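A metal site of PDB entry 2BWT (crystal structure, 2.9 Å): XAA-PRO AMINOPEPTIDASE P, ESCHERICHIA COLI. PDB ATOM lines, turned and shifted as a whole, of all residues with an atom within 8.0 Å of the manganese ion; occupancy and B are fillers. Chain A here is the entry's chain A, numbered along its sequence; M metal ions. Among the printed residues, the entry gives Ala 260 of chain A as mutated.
The side-chain carboxylate (OD1) of Asp 271 sits at hydrogen-bond distance from the side-chain hydroxyl (OH) of Tyr 229 (2.7 Å).
The backbone NH (N) of Asp 271 is in hydrogen-bond range of the side-chain carboxylate (OD2) of Asp 408 (3.1 Å).
The side-chain hydroxyl of Thr 273 sits at hydrogen-bond distance from the side-chain carboxylate of Glu 406 (2.7 Å).
The side-chain carboxylate of Glu 383 sits close to the side-chain hydroxyl of Thr 381 (2.7 Å).
The backbone carbonyl oxygen (O) of Leu 352 sits at hydrogen-bond distance from the backbone NH (N) of Glu 383.
The backbone carbonyl oxygen (O) of His 354 sits at hydrogen-bond distance from the backbone NH (N) of Thr 381 (2.9 Å).
ND1 of His 354 sits at hydrogen-bond distance from O of Val 360, at 3.0 Å.
The side-chain hydroxyl of Ser 353 lies within hydrogen-bond range of the backbone carbonyl oxygen of Thr 381 (2.5 Å).
OG1 of Thr 381 touches the manganese ion, at 3.9 Å.
Of the 24 residues printed, 5 come within 4 Å of the manganese ion.
OD2 of Asp 271 binds the manganese ion, at 2.1 Å.
OE2 of Glu 406 is bound to the manganese ion (2.2 Å).
The manganese ion is bound by OE2 of Glu 383 (2.2 Å).
NE2 of His 354 is bound to the manganese ion (2.2 Å).
The manganese ion has four donor atoms within binding distance.
Slightly farther from the manganese ion lies OE1 of Glu 406 (2.9 Å).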
ATOM      1  N   TYR A 229      17.732 -28.007   0.126  1.00  0.00           N
ATOM      2  CA  TYR A 229      18.620 -29.151  -0.069  1.00  0.00           C
ATOM      3  C   TYR A 229      17.805 -30.431  -0.192  1.00  0.00           C
ATOM      4  O   TYR A 229      16.651 -30.480   0.216  1.00  0.00           O
ATOM      5  CB  TYR A 229      19.629 -29.268   1.087  1.00  0.00           C
ATOM      6  CG  TYR A 229      18.998 -29.493   2.455  1.00  0.00           C
ATOM      7  CD1 TYR A 229      18.676 -28.411   3.276  1.00  0.00           C
ATOM      8  CD2 TYR A 229      18.735 -30.778   2.914  1.00  0.00           C
ATOM      9  CE1 TYR A 229      18.101 -28.605   4.529  1.00  0.00           C
ATOM     10  CE2 TYR A 229      18.145 -30.986   4.165  1.00  0.00           C
ATOM     11  CZ  TYR A 229      17.839 -29.888   4.959  1.00  0.00           C
ATOM     12  OH  TYR A 229      17.261 -30.093   6.204  1.00  0.00           O
ATOM     13  N   HIS A 243      23.763 -38.160   5.114  1.00  0.00           N
ATOM     14  CA  HIS A 243      23.136 -37.703   3.879  1.00  0.00           C
ATOM     15  C   HIS A 243      22.490 -38.915   3.171  1.00  0.00           C
ATOM     16  O   HIS A 243      22.921 -39.380   2.102  1.00  0.00           O
ATOM     17  CB  HIS A 243      24.134 -36.917   3.007  1.00  0.00           C
ATOM     18  CG  HIS A 243      24.622 -35.645   3.645  1.00  0.00           C
ATOM     19  ND1 HIS A 243      25.968 -35.379   3.856  1.00  0.00           N
ATOM     20  CD2 HIS A 243      23.959 -34.571   4.146  1.00  0.00           C
ATOM     21  CE1 HIS A 243      26.101 -34.208   4.447  1.00  0.00           C
ATOM     22  NE2 HIS A 243      24.899 -33.691   4.632  1.00  0.00           N
ATOM     23  N   ALA A 260      15.135 -34.583   7.902  1.00  0.00           N
ATOM     24  CA  ALA A 260      15.897 -33.371   7.688  1.00  0.00           C
ATOM     25  C   ALA A 260      15.414 -32.731   6.395  1.00  0.00           C
ATOM     26  O   ALA A 260      15.696 -33.217   5.297  1.00  0.00           O
ATOM     27  CB  ALA A 260      17.388 -33.674   7.626  1.00  0.00           C
ATOM     28  N   GLY A 270      15.563 -22.433   4.929  1.00  0.00           N
ATOM     29  CA  GLY A 270      15.245 -23.035   6.205  1.00  0.00           C
ATOM     30  C   GLY A 270      15.980 -24.348   6.240  1.00  0.00           C
ATOM     31  O   GLY A 270      16.287 -24.919   5.197  1.00  0.00           O
ATOM     32  N   ASP A 271      16.290 -24.828   7.447  1.00  0.00           N
ATOM     33  CA  ASP A 271      16.958 -26.121   7.653  1.00  0.00           C
ATOM     34  C   ASP A 271      16.608 -26.640   9.045  1.00  0.00           C
ATOM     35  O   ASP A 271      17.120 -26.151  10.051  1.00  0.00           O
ATOM     36  CB  ASP A 271      18.479 -25.970   7.485  1.00  0.00           C
ATOM     37  CG  ASP A 271      19.247 -27.268   7.759  1.00  0.00           C
ATOM     38  OD1 ASP A 271      18.622 -28.348   7.795  1.00  0.00           O
ATOM     39  OD2 ASP A 271      20.483 -27.197   7.948  1.00  0.00           O
ATOM     40  N   ILE A 272      15.707 -27.610   9.092  1.00  0.00           N
ATOM     41  CA  ILE A 272      15.250 -28.196  10.336  1.00  0.00           C
ATOM     42  C   ILE A 272      15.475 -29.699  10.280  1.00  0.00           C
ATOM     43  O   ILE A 272      15.291 -30.324   9.233  1.00  0.00           O
ATOM     44  CB  ILE A 272      13.745 -27.920  10.565  1.00  0.00           C
ATOM     45  CG1 ILE A 272      13.499 -26.447  10.853  1.00  0.00           C
ATOM     46  CG2 ILE A 272      13.184 -28.763  11.738  1.00  0.00           C
ATOM     47  CD1 ILE A 272      12.029 -26.132  11.066  1.00  0.00           C
ATOM     48  N   THR A 273      15.857 -30.271  11.428  1.00  0.00           N
ATOM     49  CA  THR A 273      15.877 -31.712  11.628  1.00  0.00           C
ATOM     50  C   THR A 273      15.012 -32.054  12.838  1.00  0.00           C
ATOM     51  O   THR A 273      15.109 -31.399  13.863  1.00  0.00           O
ATOM     52  CB  THR A 273      17.283 -32.265  11.889  1.00  0.00           C
ATOM     53  OG1 THR A 273      18.211 -31.700  10.959  1.00  0.00           O
ATOM     54  CG2 THR A 273      17.292 -33.775  11.738  1.00  0.00           C
ATOM     55  N   HIS A 350      29.799 -34.731  13.343  1.00  0.00           N
ATOM     56  CA  HIS A 350      29.735 -33.489  12.582  1.00  0.00           C
ATOM     57  C   HIS A 350      29.727 -32.304  13.541  1.00  0.00           C
ATOM     58  O   HIS A 350      29.746 -32.483  14.753  1.00  0.00           O
ATOM     59  CB  HIS A 350      28.530 -33.473  11.642  1.00  0.00           C
ATOM     60  CG  HIS A 350      27.214 -33.657  12.334  1.00  0.00           C
ATOM     61  ND1 HIS A 350      26.518 -32.618  12.901  1.00  0.00           N
ATOM     62  CD2 HIS A 350      26.470 -34.778  12.532  1.00  0.00           C
ATOM     63  CE1 HIS A 350      25.395 -33.088  13.437  1.00  0.00           C
ATOM     64  NE2 HIS A 350      25.341 -34.386  13.224  1.00  0.00           N
ATOM     65  N   GLY A 351      29.725 -31.093  12.985  1.00  0.00           N
ATOM     66  CA  GLY A 351      29.693 -29.865  13.770  1.00  0.00           C
ATOM     67  C   GLY A 351      28.343 -29.609  14.416  1.00  0.00           C
ATOM     68  O   GLY A 351      27.331 -30.217  14.040  1.00  0.00           O
ATOM     69  N   LEU A 352      28.340 -28.699  15.384  1.00  0.00           N
ATOM     70  CA  LEU A 352      27.121 -28.329  16.098  1.00  0.00           C
ATOM     71  C   LEU A 352      26.275 -27.337  15.306  1.00  0.00           C
ATOM     72  O   LEU A 352      25.042 -27.350  15.402  1.00  0.00           O
ATOM     73  CB  LEU A 352      27.467 -27.699  17.458  1.00  0.00           C
ATOM     74  CG  LEU A 352      26.271 -27.240  18.320  1.00  0.00           C
ATOM     75  CD1 LEU A 352      25.337 -28.403  18.634  1.00  0.00           C
ATOM     76  CD2 LEU A 352      26.733 -26.579  19.602  1.00  0.00           C
ATOM     77  N   SER A 353      26.927 -26.482  14.530  1.00  0.00           N
ATOM     78  CA  SER A 353      26.268 -25.322  13.930  1.00  0.00           C
ATOM     79  C   SER A 353      26.927 -24.921  12.620  1.00  0.00           C
ATOM     80  O   SER A 353      28.133 -24.968  12.516  1.00  0.00           O
ATOM     81  CB  SER A 353      26.324 -24.120  14.893  1.00  0.00           C
ATOM     82  OG  SER A 353      25.495 -24.305  16.031  1.00  0.00           O
ATOM     83  N   HIS A 354      26.114 -24.534  11.640  1.00  0.00           N
ATOM     84  CA  HIS A 354      26.601 -23.924  10.414  1.00  0.00           C
ATOM     85  C   HIS A 354      25.834 -22.649  10.088  1.00  0.00           C
ATOM     86  O   HIS A 354      24.652 -22.527  10.417  1.00  0.00           O
ATOM     87  CB  HIS A 354      26.566 -24.890   9.203  1.00  0.00           C
ATOM     88  CG  HIS A 354      25.211 -25.438   8.865  1.00  0.00           C
ATOM     89  ND1 HIS A 354      24.290 -24.754   8.103  1.00  0.00           N
ATOM     90  CD2 HIS A 354      24.648 -26.645   9.137  1.00  0.00           C
ATOM     91  CE1 HIS A 354      23.212 -25.493   7.951  1.00  0.00           C
ATOM     92  NE2 HIS A 354      23.390 -26.644   8.571  1.00  0.00           N
ATOM     93  N   TRP A 355      26.530 -21.713   9.452  1.00  0.00           N
ATOM     94  CA  TRP A 355      25.910 -20.491   8.946  1.00  0.00           C
ATOM     95  C   TRP A 355      24.717 -20.841   8.047  1.00  0.00           C
ATOM     96  O   TRP A 355      24.758 -21.833   7.298  1.00  0.00           O
ATOM     97  CB  TRP A 355      26.920 -19.663   8.123  1.00  0.00           C
ATOM     98  CG  TRP A 355      28.230 -19.278   8.810  1.00  0.00           C
ATOM     99  CD1 TRP A 355      29.482 -19.338   8.263  1.00  0.00           C
ATOM    100  CD2 TRP A 355      28.400 -18.728  10.131  1.00  0.00           C
ATOM    101  NE1 TRP A 355      30.417 -18.882   9.159  1.00  0.00           N
ATOM    102  CE2 TRP A 355      29.784 -18.503  10.309  1.00  0.00           C
ATOM    103  CE3 TRP A 355      27.524 -18.433  11.177  1.00  0.00           C
ATOM    104  CZ2 TRP A 355      30.315 -17.988  11.498  1.00  0.00           C
ATOM    105  CZ3 TRP A 355      28.047 -17.906  12.352  1.00  0.00           C
ATOM    106  CH2 TRP A 355      29.434 -17.694  12.500  1.00  0.00           C
ATOM    107  N   LEU A 356      23.663 -20.039   8.100  1.00  0.00           N
ATOM    108  CA  LEU A 356      22.480 -20.255   7.261  1.00  0.00           C
ATOM    109  C   LEU A 356      22.147 -18.970   6.488  1.00  0.00           C
ATOM    110  O   LEU A 356      22.285 -17.873   7.021  1.00  0.00           O
ATOM    111  CB  LEU A 356      21.300 -20.666   8.137  1.00  0.00           C
ATOM    112  CG  LEU A 356      19.986 -21.131   7.482  1.00  0.00           C
ATOM    113  CD1 LEU A 356      20.151 -22.465   6.753  1.00  0.00           C
ATOM    114  CD2 LEU A 356      18.904 -21.237   8.556  1.00  0.00           C
ATOM    115  N   VAL A 360      22.155 -23.057   2.297  1.00  0.00           N
ATOM    116  CA  VAL A 360      21.897 -23.747   3.571  1.00  0.00           C
ATOM    117  C   VAL A 360      23.203 -23.878   4.379  1.00  0.00           C
ATOM    118  O   VAL A 360      23.240 -23.540   5.570  1.00  0.00           O
ATOM    119  CB  VAL A 360      21.153 -25.102   3.390  1.00  0.00           C
ATOM    120  CG1 VAL A 360      21.971 -26.110   2.604  1.00  0.00           C
ATOM    121  CG2 VAL A 360      20.776 -25.675   4.732  1.00  0.00           C
ATOM    122  N   HIS A 361      24.271 -24.345   3.733  1.00  0.00           N
ATOM    123  CA  HIS A 361      25.591 -24.287   4.330  1.00  0.00           C
ATOM    124  C   HIS A 361      26.222 -22.962   3.911  1.00  0.00           C
ATOM    125  O   HIS A 361      26.987 -22.904   2.955  1.00  0.00           O
ATOM    126  CB  HIS A 361      26.449 -25.479   3.893  1.00  0.00           C
ATOM    127  CG  HIS A 361      26.016 -26.775   4.501  1.00  0.00           C
ATOM    128  ND1 HIS A 361      26.114 -27.976   3.835  1.00  0.00           N
ATOM    129  CD2 HIS A 361      25.450 -27.050   5.701  1.00  0.00           C
ATOM    130  CE1 HIS A 361      25.636 -28.944   4.604  1.00  0.00           C
ATOM    131  NE2 HIS A 361      25.224 -28.405   5.746  1.00  0.00           N
ATOM    132  N   LEU A 380      22.459 -18.997  12.107  1.00  0.00           N
ATOM    133  CA  LEU A 380      23.121 -20.291  12.178  1.00  0.00           C
ATOM    134  C   LEU A 380      22.158 -21.358  12.695  1.00  0.00           C
ATOM    135  O   LEU A 380      21.132 -21.048  13.316  1.00  0.00           O
ATOM    136  CB  LEU A 380      24.374 -20.213  13.053  1.00  0.00           C
ATOM    137  CG  LEU A 380      24.170 -19.903  14.545  1.00  0.00           C
ATOM    138  CD1 LEU A 380      25.414 -20.288  15.334  1.00  0.00           C
ATOM    139  CD2 LEU A 380      23.835 -18.428  14.801  1.00  0.00           C
ATOM    140  N   THR A 381      22.517 -22.606  12.411  1.00  0.00           N
ATOM    141  CA  THR A 381      21.765 -23.775  12.859  1.00  0.00           C
ATOM    142  C   THR A 381      22.362 -24.300  14.157  1.00  0.00           C
ATOM    143  O   THR A 381      23.541 -24.083  14.447  1.00  0.00           O
ATOM    144  CB  THR A 381      21.785 -24.895  11.802  1.00  0.00           C
ATOM    145  OG1 THR A 381      23.087 -25.507  11.752  1.00  0.00           O
ATOM    146  CG2 THR A 381      21.427 -24.346  10.431  1.00  0.00           C
ATOM    147  N   VAL A 382      21.525 -24.953  14.958  1.00  0.00           N
ATOM    148  CA  VAL A 382      21.962 -25.635  16.180  1.00  0.00           C
ATOM    149  C   VAL A 382      21.498 -27.059  15.994  1.00  0.00           C
ATOM    150  O   VAL A 382      20.292 -27.309  15.998  1.00  0.00           O
ATOM    151  CB  VAL A 382      21.296 -25.016  17.444  1.00  0.00           C
ATOM    152  CG1 VAL A 382      22.018 -25.497  18.702  1.00  0.00           C
ATOM    153  CG2 VAL A 382      21.304 -23.489  17.370  1.00  0.00           C
ATOM    154  N   GLU A 383      22.430 -27.990  15.806  1.00  0.00           N
ATOM    155  CA  GLU A 383      22.071 -29.357  15.374  1.00  0.00           C
ATOM    156  C   GLU A 383      22.931 -30.461  15.989  1.00  0.00           C
ATOM    157  O   GLU A 383      23.712 -31.108  15.281  1.00  0.00           O
ATOM    158  CB  GLU A 383      22.088 -29.451  13.845  1.00  0.00           C
ATOM    159  CG  GLU A 383      23.400 -29.103  13.144  1.00  0.00           C
ATOM    160  CD  GLU A 383      23.277 -29.140  11.623  1.00  0.00           C
ATOM    161  OE1 GLU A 383      23.498 -30.215  11.014  1.00  0.00           O
ATOM    162  OE2 GLU A 383      22.971 -28.088  11.008  1.00  0.00           O
ATOM    163  N   ARG A 404      18.868 -36.714  15.446  1.00  0.00           N
ATOM    164  CA  ARG A 404      19.291 -35.315  15.420  1.00  0.00           C
ATOM    165  C   ARG A 404      18.078 -34.407  15.603  1.00  0.00           C
ATOM    166  O   ARG A 404      16.986 -34.731  15.138  1.00  0.00           O
ATOM    167  CB  ARG A 404      20.000 -34.974  14.112  1.00  0.00           C
ATOM    168  CG  ARG A 404      20.551 -33.539  14.082  1.00  0.00           C
ATOM    169  CD  ARG A 404      21.497 -33.252  12.904  1.00  0.00           C
ATOM    170  NE  ARG A 404      20.793 -33.246  11.624  1.00  0.00           N
ATOM    171  CZ  ARG A 404      20.908 -34.184  10.678  1.00  0.00           C
ATOM    172  NH1 ARG A 404      21.706 -35.230  10.820  1.00  0.00           N
ATOM    173  NH2 ARG A 404      20.196 -34.070   9.568  1.00  0.00           N
ATOM    174  N   GLU A 406      17.419 -30.227  15.076  1.00  0.00           N
ATOM    175  CA  GLU A 406      18.044 -29.019  14.550  1.00  0.00           C
ATOM    176  C   GLU A 406      17.055 -27.876  14.534  1.00  0.00           C
ATOM    177  O   GLU A 406      15.929 -28.035  14.081  1.00  0.00           O
ATOM    178  CB  GLU A 406      18.600 -29.262  13.135  1.00  0.00           C
ATOM    179  CG  GLU A 406      18.999 -28.007  12.357  1.00  0.00           C
ATOM    180  CD  GLU A 406      19.716 -28.319  11.047  1.00  0.00           C
ATOM    181  OE1 GLU A 406      19.626 -29.461  10.531  1.00  0.00           O
ATOM    182  OE2 GLU A 406      20.389 -27.404  10.514  1.00  0.00           O
ATOM    183  N   ASP A 407      17.518 -26.725  15.042  1.00  0.00           N
ATOM    184  CA  ASP A 407      16.788 -25.461  14.987  1.00  0.00           C
ATOM    185  C   ASP A 407      17.647 -24.410  14.278  1.00  0.00           C
ATOM    186  O   ASP A 407      18.876 -24.502  14.269  1.00  0.00           O
ATOM    187  CB  ASP A 407      16.453 -24.967  16.405  1.00  0.00           C
ATOM    188  CG  ASP A 407      15.109 -25.482  16.919  1.00  0.00           C
ATOM    189  OD1 ASP A 407      14.293 -25.988  16.129  1.00  0.00           O
ATOM    190  OD2 ASP A 407      14.870 -25.352  18.139  1.00  0.00           O
ATOM    191  N   ASP A 408      16.990 -23.398  13.702  1.00  0.00           N
ATOM    192  CA  ASP A 408      17.657 -22.232  13.122  1.00  0.00           C
ATOM    193  C   ASP A 408      17.484 -21.015  14.036  1.00  0.00           C
ATOM    194  O   ASP A 408      16.365 -20.681  14.436  1.00  0.00           O
ATOM    195  CB  ASP A 408      17.070 -21.942  11.746  1.00  0.00           C
ATOM    196  CG  ASP A 408      17.065 -23.153  10.848  1.00  0.00           C
ATOM    197  OD1 ASP A 408      18.044 -23.924  10.873  1.00  0.00           O
ATOM    198  OD2 ASP A 408      16.081 -23.340  10.104  1.00  0.00           O
HETATM  199 MN    MN M   1      21.865 -28.144   9.136  1.00  0.00          MN
